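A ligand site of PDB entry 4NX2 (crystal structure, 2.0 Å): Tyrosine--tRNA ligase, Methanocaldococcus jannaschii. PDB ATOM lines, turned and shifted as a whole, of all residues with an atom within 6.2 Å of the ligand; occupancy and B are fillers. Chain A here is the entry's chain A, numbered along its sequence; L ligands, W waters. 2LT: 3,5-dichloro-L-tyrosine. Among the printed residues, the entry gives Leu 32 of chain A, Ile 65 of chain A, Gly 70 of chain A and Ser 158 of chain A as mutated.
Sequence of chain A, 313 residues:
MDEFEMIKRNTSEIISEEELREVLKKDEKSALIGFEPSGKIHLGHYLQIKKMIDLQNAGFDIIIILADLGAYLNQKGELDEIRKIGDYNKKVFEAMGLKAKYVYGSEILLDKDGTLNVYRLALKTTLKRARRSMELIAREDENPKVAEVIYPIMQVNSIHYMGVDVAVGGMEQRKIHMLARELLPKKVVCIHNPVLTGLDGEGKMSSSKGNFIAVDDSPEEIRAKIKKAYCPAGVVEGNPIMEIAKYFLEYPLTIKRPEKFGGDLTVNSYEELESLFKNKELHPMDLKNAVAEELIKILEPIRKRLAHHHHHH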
ATOM      1  N   LEU A  32     -13.397  18.377  -0.720  1.00  0.00           N
ATOM      2  CA  LEU A  32     -13.365  17.135   0.043  1.00  0.00           C
ATOM      3  C   LEU A  32     -14.659  16.865   0.771  1.00  0.00           C
ATOM      4  O   LEU A  32     -15.466  17.769   1.015  1.00  0.00           O
ATOM      5  CB  LEU A  32     -12.156  17.073   0.988  1.00  0.00           C
ATOM      6  CG  LEU A  32     -12.048  17.757   2.351  1.00  0.00           C
ATOM      7  CD1 LEU A  32     -12.955  17.151   3.407  1.00  0.00           C
ATOM      8  CD2 LEU A  32     -10.614  17.702   2.856  1.00  0.00           C
ATOM      9  N   ILE A  33     -14.875  15.597   1.087  1.00  0.00           N
ATOM     10  CA  ILE A  33     -15.866  15.204   2.069  1.00  0.00           C
ATOM     11  C   ILE A  33     -15.197  14.098   2.869  1.00  0.00           C
ATOM     12  O   ILE A  33     -14.332  13.381   2.335  1.00  0.00           O
ATOM     13  CB  ILE A  33     -17.178  14.711   1.392  1.00  0.00           C
ATOM     14  CG1 ILE A  33     -18.226  14.332   2.448  1.00  0.00           C
ATOM     15  CG2 ILE A  33     -16.909  13.555   0.438  1.00  0.00           C
ATOM     16  CD1 ILE A  33     -19.634  14.168   1.859  1.00  0.00           C
ATOM     17  N   GLY A  34     -15.544  13.971   4.155  1.00  0.00           N
ATOM     18  CA  GLY A  34     -15.053  12.866   4.950  1.00  0.00           C
ATOM     19  C   GLY A  34     -16.186  11.973   5.424  1.00  0.00           C
ATOM     20  O   GLY A  34     -17.292  12.439   5.667  1.00  0.00           O
ATOM     21  N   PHE A  35     -15.925  10.671   5.530  1.00  0.00           N
ATOM     22  CA  PHE A  35     -16.886   9.741   6.092  1.00  0.00           C
ATOM     23  C   PHE A  35     -16.242   8.863   7.164  1.00  0.00           C
ATOM     24  O   PHE A  35     -15.168   8.301   6.935  1.00  0.00           O
ATOM     25  CB  PHE A  35     -17.383   8.777   5.007  1.00  0.00           C
ATOM     26  CG  PHE A  35     -18.156   9.429   3.895  1.00  0.00           C
ATOM     27  CD1 PHE A  35     -19.465   9.828   4.085  1.00  0.00           C
ATOM     28  CD2 PHE A  35     -17.580   9.583   2.649  1.00  0.00           C
ATOM     29  CE1 PHE A  35     -20.182  10.405   3.037  1.00  0.00           C
ATOM     30  CE2 PHE A  35     -18.285  10.152   1.603  1.00  0.00           C
ATOM     31  CZ  PHE A  35     -19.591  10.570   1.804  1.00  0.00           C
ATOM     32  N   GLU A  36     -16.903   8.704   8.304  1.00  0.00           N
ATOM     33  CA  GLU A  36     -16.558   7.593   9.190  1.00  0.00           C
ATOM     34  C   GLU A  36     -16.879   6.326   8.400  1.00  0.00           C
ATOM     35  O   GLU A  36     -17.992   6.198   7.878  1.00  0.00           O
ATOM     36  CB  GLU A  36     -17.387   7.632  10.467  1.00  0.00           C
ATOM     37  CG  GLU A  36     -17.084   8.863  11.358  1.00  0.00           C
ATOM     38  CD  GLU A  36     -17.734   8.782  12.727  1.00  0.00           C
ATOM     39  OE1 GLU A  36     -18.066   7.658  13.158  1.00  0.00           O
ATOM     40  OE2 GLU A  36     -17.924   9.851  13.365  1.00  0.00           O
ATOM     41  N   ILE A  65     -12.009  11.717   2.375  1.00  0.00           N
ATOM     42  CA  ILE A  65     -11.335  11.312   3.599  1.00  0.00           C
ATOM     43  C   ILE A  65     -12.053  10.109   4.198  1.00  0.00           C
ATOM     44  O   ILE A  65     -13.248  10.181   4.513  1.00  0.00           O
ATOM     45  CB  ILE A  65     -11.297  12.453   4.631  1.00  0.00           C
ATOM     46  CG1 ILE A  65     -10.510  13.652   4.088  1.00  0.00           C
ATOM     47  CG2 ILE A  65     -10.678  11.963   5.954  1.00  0.00           C
ATOM     48  CD1 ILE A  65      -9.015  13.530   4.259  1.00  0.00           C
ATOM     49  N   ALA A  67     -12.380   8.577   7.363  1.00  0.00           N
ATOM     50  CA  ALA A  67     -12.051   9.106   8.685  1.00  0.00           C
ATOM     51  C   ALA A  67     -11.878   7.991   9.714  1.00  0.00           C
ATOM     52  O   ALA A  67     -12.722   7.818  10.606  1.00  0.00           O
ATOM     53  CB  ALA A  67     -13.110  10.079   9.135  1.00  0.00           C
ATOM     54  N   LEU A  69      -9.497   7.584  12.130  1.00  0.00           N
ATOM     55  CA  LEU A  69      -9.213   8.060  13.477  1.00  0.00           C
ATOM     56  C   LEU A  69     -10.469   8.677  14.063  1.00  0.00           C
ATOM     57  O   LEU A  69     -10.810   8.436  15.230  1.00  0.00           O
ATOM     58  CB  LEU A  69      -8.062   9.058  13.469  1.00  0.00           C
ATOM     59  CG  LEU A  69      -6.799   8.645  14.214  1.00  0.00           C
ATOM     60  CD1 LEU A  69      -6.629   7.133  14.233  1.00  0.00           C
ATOM     61  CD2 LEU A  69      -5.566   9.281  13.582  1.00  0.00           C
ATOM     62  N   GLY A  70     -11.172   9.449  13.233  1.00  0.00           N
ATOM     63  CA  GLY A  70     -12.443  10.028  13.632  1.00  0.00           C
ATOM     64  C   GLY A  70     -13.414   8.959  14.104  1.00  0.00           C
ATOM     65  O   GLY A  70     -14.002   9.083  15.194  1.00  0.00           O
ATOM     66  N   ALA A  71     -13.576   7.912  13.310  1.00  0.00           N
ATOM     67  CA  ALA A  71     -14.485   6.851  13.667  1.00  0.00           C
ATOM     68  C   ALA A  71     -14.001   6.152  14.950  1.00  0.00           C
ATOM     69  O   ALA A  71     -14.800   5.848  15.836  1.00  0.00           O
ATOM     70  CB  ALA A  71     -14.611   5.863  12.521  1.00  0.00           C
ATOM     71  N   GLY A 105      -7.733   9.469   7.304  1.00  0.00           N
ATOM     72  CA  GLY A 105      -7.475  10.575   8.208  1.00  0.00           C
ATOM     73  C   GLY A 105      -6.219  10.321   9.026  1.00  0.00           C
ATOM     74  O   GLY A 105      -5.487  11.245   9.348  1.00  0.00           O
ATOM     75  N   ILE A 137     -23.244  14.718  16.082  1.00  0.00           N
ATOM     76  CA  ILE A 137     -22.277  13.778  15.581  1.00  0.00           C
ATOM     77  C   ILE A 137     -21.870  12.689  16.569  1.00  0.00           C
ATOM     78  O   ILE A 137     -21.800  11.564  16.224  1.00  0.00           O
ATOM     79  CB  ILE A 137     -21.045  14.522  15.076  1.00  0.00           C
ATOM     80  CG1 ILE A 137     -21.415  15.324  13.848  1.00  0.00           C
ATOM     81  CG2 ILE A 137     -19.866  13.608  14.766  1.00  0.00           C
ATOM     82  CD1 ILE A 137     -20.392  16.310  13.438  1.00  0.00           C
ATOM     83  N   TYR A 151     -11.970  15.156  18.046  1.00  0.00           N
ATOM     84  CA  TYR A 151     -12.619  14.864  16.764  1.00  0.00           C
ATOM     85  C   TYR A 151     -12.810  16.089  15.857  1.00  0.00           C
ATOM     86  O   TYR A 151     -12.333  16.089  14.709  1.00  0.00           O
ATOM     87  CB  TYR A 151     -13.951  14.134  17.027  1.00  0.00           C
ATOM     88  CG  TYR A 151     -14.740  13.619  15.828  1.00  0.00           C
ATOM     89  CD1 TYR A 151     -15.391  14.496  14.954  1.00  0.00           C
ATOM     90  CD2 TYR A 151     -14.923  12.265  15.629  1.00  0.00           C
ATOM     91  CE1 TYR A 151     -16.155  14.020  13.887  1.00  0.00           C
ATOM     92  CE2 TYR A 151     -15.673  11.775  14.571  1.00  0.00           C
ATOM     93  CZ  TYR A 151     -16.291  12.651  13.707  1.00  0.00           C
ATOM     94  OH  TYR A 151     -17.051  12.138  12.664  1.00  0.00           O
ATOM     95  N   PRO A 152     -13.502  17.149  16.335  1.00  0.00           N
ATOM     96  CA  PRO A 152     -13.698  18.269  15.412  1.00  0.00           C
ATOM     97  C   PRO A 152     -12.398  18.954  14.977  1.00  0.00           C
ATOM     98  O   PRO A 152     -12.328  19.449  13.852  1.00  0.00           O
ATOM     99  CB  PRO A 152     -14.569  19.251  16.221  1.00  0.00           C
ATOM    100  CG  PRO A 152     -14.325  18.873  17.653  1.00  0.00           C
ATOM    101  CD  PRO A 152     -14.164  17.389  17.645  1.00  0.00           C
ATOM    102  N   MET A 154      -9.557  17.503  14.527  1.00  0.00           N
ATOM    103  CA  MET A 154      -9.010  16.654  13.482  1.00  0.00           C
ATOM    104  C   MET A 154      -9.624  16.933  12.130  1.00  0.00           C
ATOM    105  O   MET A 154      -8.920  16.991  11.121  1.00  0.00           O
ATOM    106  CB  MET A 154      -9.184  15.179  13.832  1.00  0.00           C
ATOM    107  CG  MET A 154      -8.134  14.689  14.795  1.00  0.00           C
ATOM    108  SD  MET A 154      -8.789  13.337  15.768  1.00  0.00           S
ATOM    109  CE  MET A 154      -9.309  12.241  14.449  1.00  0.00           C
ATOM    110  N   GLN A 155     -10.940  17.121  12.101  1.00  0.00           N
ATOM    111  CA  GLN A 155     -11.627  17.383  10.838  1.00  0.00           C
ATOM    112  C   GLN A 155     -11.206  18.733  10.272  1.00  0.00           C
ATOM    113  O   GLN A 155     -10.994  18.877   9.062  1.00  0.00           O
ATOM    114  CB  GLN A 155     -13.142  17.343  11.060  1.00  0.00           C
ATOM    115  CG  GLN A 155     -13.953  17.283   9.766  1.00  0.00           C
ATOM    116  CD  GLN A 155     -15.399  16.852   9.988  1.00  0.00           C
ATOM    117  OE1 GLN A 155     -15.703  16.157  10.958  1.00  0.00           O
ATOM    118  NE2 GLN A 155     -16.292  17.270   9.097  1.00  0.00           N
ATOM    119  N   VAL A 156     -11.066  19.733  11.135  1.00  0.00           N
ATOM    120  CA  VAL A 156     -10.607  21.054  10.687  1.00  0.00           C
ATOM    121  C   VAL A 156      -9.207  20.936  10.126  1.00  0.00           C
ATOM    122  O   VAL A 156      -8.893  21.510   9.082  1.00  0.00           O
ATOM    123  CB  VAL A 156     -10.613  22.094  11.840  1.00  0.00           C
ATOM    124  CG1 VAL A 156      -9.965  23.405  11.401  1.00  0.00           C
ATOM    125  CG2 VAL A 156     -12.036  22.341  12.332  1.00  0.00           C
ATOM    126  N   SER A 158      -7.778  18.281   8.718  1.00  0.00           N
ATOM    127  CA  SER A 158      -7.806  17.578   7.433  1.00  0.00           C
ATOM    128  C   SER A 158      -8.162  18.538   6.307  1.00  0.00           C
ATOM    129  O   SER A 158      -7.569  18.495   5.230  1.00  0.00           O
ATOM    130  CB  SER A 158      -8.833  16.427   7.447  1.00  0.00           C
ATOM    131  OG  SER A 158      -8.496  15.467   8.427  1.00  0.00           O
ATOM    132  N   ILE A 159      -9.136  19.402   6.564  1.00  0.00           N
ATOM    133  CA  ILE A 159      -9.509  20.417   5.575  1.00  0.00           C
ATOM    134  C   ILE A 159      -8.292  21.283   5.225  1.00  0.00           C
ATOM    135  O   ILE A 159      -8.004  21.525   4.057  1.00  0.00           O
ATOM    136  CB  ILE A 159     -10.659  21.324   6.100  1.00  0.00           C
ATOM    137  CG1 ILE A 159     -11.988  20.567   6.071  1.00  0.00           C
ATOM    138  CG2 ILE A 159     -10.750  22.604   5.275  1.00  0.00           C
ATOM    139  CD1 ILE A 159     -13.115  21.262   6.832  1.00  0.00           C
ATOM    140  N   GLU A 172     -25.379  18.215   9.548  1.00  0.00           N
ATOM    141  CA  GLU A 172     -24.838  17.955  10.882  1.00  0.00           C
ATOM    142  C   GLU A 172     -23.371  18.429  11.043  1.00  0.00           C
ATOM    143  O   GLU A 172     -22.914  18.713  12.151  1.00  0.00           O
ATOM    144  CB  GLU A 172     -24.982  16.477  11.255  1.00  0.00           C
ATOM    145  CG  GLU A 172     -23.967  15.549  10.584  1.00  0.00           C
ATOM    146  CD  GLU A 172     -24.334  15.202   9.144  1.00  0.00           C
ATOM    147  OE1 GLU A 172     -25.534  15.361   8.780  1.00  0.00           O
ATOM    148  OE2 GLU A 172     -23.432  14.754   8.385  1.00  0.00           O
ATOM    149  N   GLN A 173     -22.657  18.533   9.918  1.00  0.00           N
ATOM    150  CA  GLN A 173     -21.270  19.018   9.917  1.00  0.00           C
ATOM    151  C   GLN A 173     -21.139  20.544   9.985  1.00  0.00           C
ATOM    152  O   GLN A 173     -20.010  21.052   9.966  1.00  0.00           O
ATOM    153  CB  GLN A 173     -20.539  18.549   8.653  1.00  0.00           C
ATOM    154  CG  GLN A 173     -20.604  17.057   8.356  1.00  0.00           C
ATOM    155  CD  GLN A 173     -20.020  16.230   9.478  1.00  0.00           C
ATOM    156  OE1 GLN A 173     -18.920  16.520   9.960  1.00  0.00           O
ATOM    157  NE2 GLN A 173     -20.754  15.206   9.920  1.00  0.00           N
ATOM    158  N   ILE A 176     -18.872  22.193  12.752  1.00  0.00           N
ATOM    159  CA  ILE A 176     -17.459  21.880  12.545  1.00  0.00           C
ATOM    160  C   ILE A 176     -16.908  22.734  11.424  1.00  0.00           C
ATOM    161  O   ILE A 176     -15.804  23.290  11.501  1.00  0.00           O
ATOM    162  CB  ILE A 176     -17.260  20.388  12.227  1.00  0.00           C
ATOM    163  CG1 ILE A 176     -17.426  19.566  13.499  1.00  0.00           C
ATOM    164  CG2 ILE A 176     -15.885  20.137  11.587  1.00  0.00           C
ATOM    165  CD1 ILE A 176     -17.240  18.046  13.285  1.00  0.00           C
HETATM  166  N   2LT L   1     -17.528  14.176  10.771  1.00  0.00           N
HETATM  167  CA  2LT L   1     -17.562  13.316   9.655  1.00  0.00           C
HETATM  168  C   2LT L   1     -18.789  12.457   9.676  1.00  0.00           C
HETATM  169  O   2LT L   1     -19.725  12.785  10.408  1.00  0.00           O
HETATM  170  CB  2LT L   1     -16.397  12.404   9.586  1.00  0.00           C
HETATM  171  CG  2LT L   1     -15.000  13.003   9.567  1.00  0.00           C
HETATM  172  CD1 2LT L   1     -14.212  12.909  10.728  1.00  0.00           C
HETATM  173  CD2 2LT L   1     -14.551  13.630   8.391  1.00  0.00           C
HETATM  174  CE1 2LT L   1     -12.899  13.456  10.700  1.00  0.00           C
HETATM  175  CE2 2LT L   1     -13.264  14.192   8.373  1.00  0.00           C
HETATM  176  CZ  2LT L   1     -12.491  14.087   9.521  1.00  0.00           C
HETATM  177  OH  2LT L   1     -11.276  14.593   9.407  1.00  0.00           O
HETATM  178  OXT 2LT L   1     -18.844  11.429   8.975  1.00  0.00           O
HETATM  179 CL1  2LT L   1     -12.046  13.369  11.926  1.00  0.00          CL
HETATM  180 CL2  2LT L   1     -12.733  14.855   7.144  1.00  0.00          CL
HETATM  181  O   HOH W   1      -9.217  13.542  10.523  1.00  0.00           O
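The side-chain amide nitrogen (NE2) of Gln 173 lies within hydrogen-bond range of an oxygen (O) of the ligand (2.7 Å).
OE1 of Gln 155 is in hydrogen-bond range of N of the ligand (2.7 Å).
A nitrogen (N) of the ligand sits at hydrogen-bond distance from the side-chain hydroxyl (OH) of Tyr 151, at 2.8 Å.
An oxygen (OH) of the ligand sits at hydrogen-bond distance from the side-chain hydroxyl (OG) of Ser 158 (3.1 Å).
An oxygen (OXT) of the ligand is in hydrogen-bond range of the backbone NH of Glu 36 (3.4 Å).
The side-chain amide nitrogen of Gln 155 lies within hydrogen-bond range of the side-chain amide oxygen of Gln 173, at 2.9 Å.
OE2 of Glu 172 lies within hydrogen-bond range of NE2 of Gln 173 (3.1 Å).
The side-chain hydroxyl (OH) of Tyr 151 is in hydrogen-bond range of the side-chain carboxylate (OE2) of Glu 36.
The side-chain hydroxyl of Ser 158 sits at hydrogen-bond distance from the backbone carbonyl oxygen of Met 154, at 3.1 Å.
N of Ala 67 sits at hydrogen-bond distance from O of Phe 35 (2.8 Å).
The backbone carbonyl oxygen (O) of Ile 65 is in hydrogen-bond range of the backbone NH (N) of Phe 35 (2.9 Å).
The backbone carbonyl oxygen (O) of Ile 33 sits at hydrogen-bond distance from the backbone NH (N) of Ile 65.
Merely in contact with the ligand: Gly 34 (3.6 Å), Phe 35 (3.9 Å), Ile 65 (3.7 Å), Ala 67 (3.4 Å), Gly 70 (3.8 Å) and Met 154 (3.8 Å).
Hydrophobic or aromatic side chains within 4 Å of the ligand: Ile 65, Ala 67, Tyr 151 and Met 154.
Of the 22 residues printed, 11 come within 4 Å of the ligand.
The nearest printed residue that does not touch the ligand is Leu 32 (4.4 Å).
Water W1 lies within hydrogen-bond range of OH of the ligand (2.6 Å) and OG of Ser 158 (2.9 Å).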
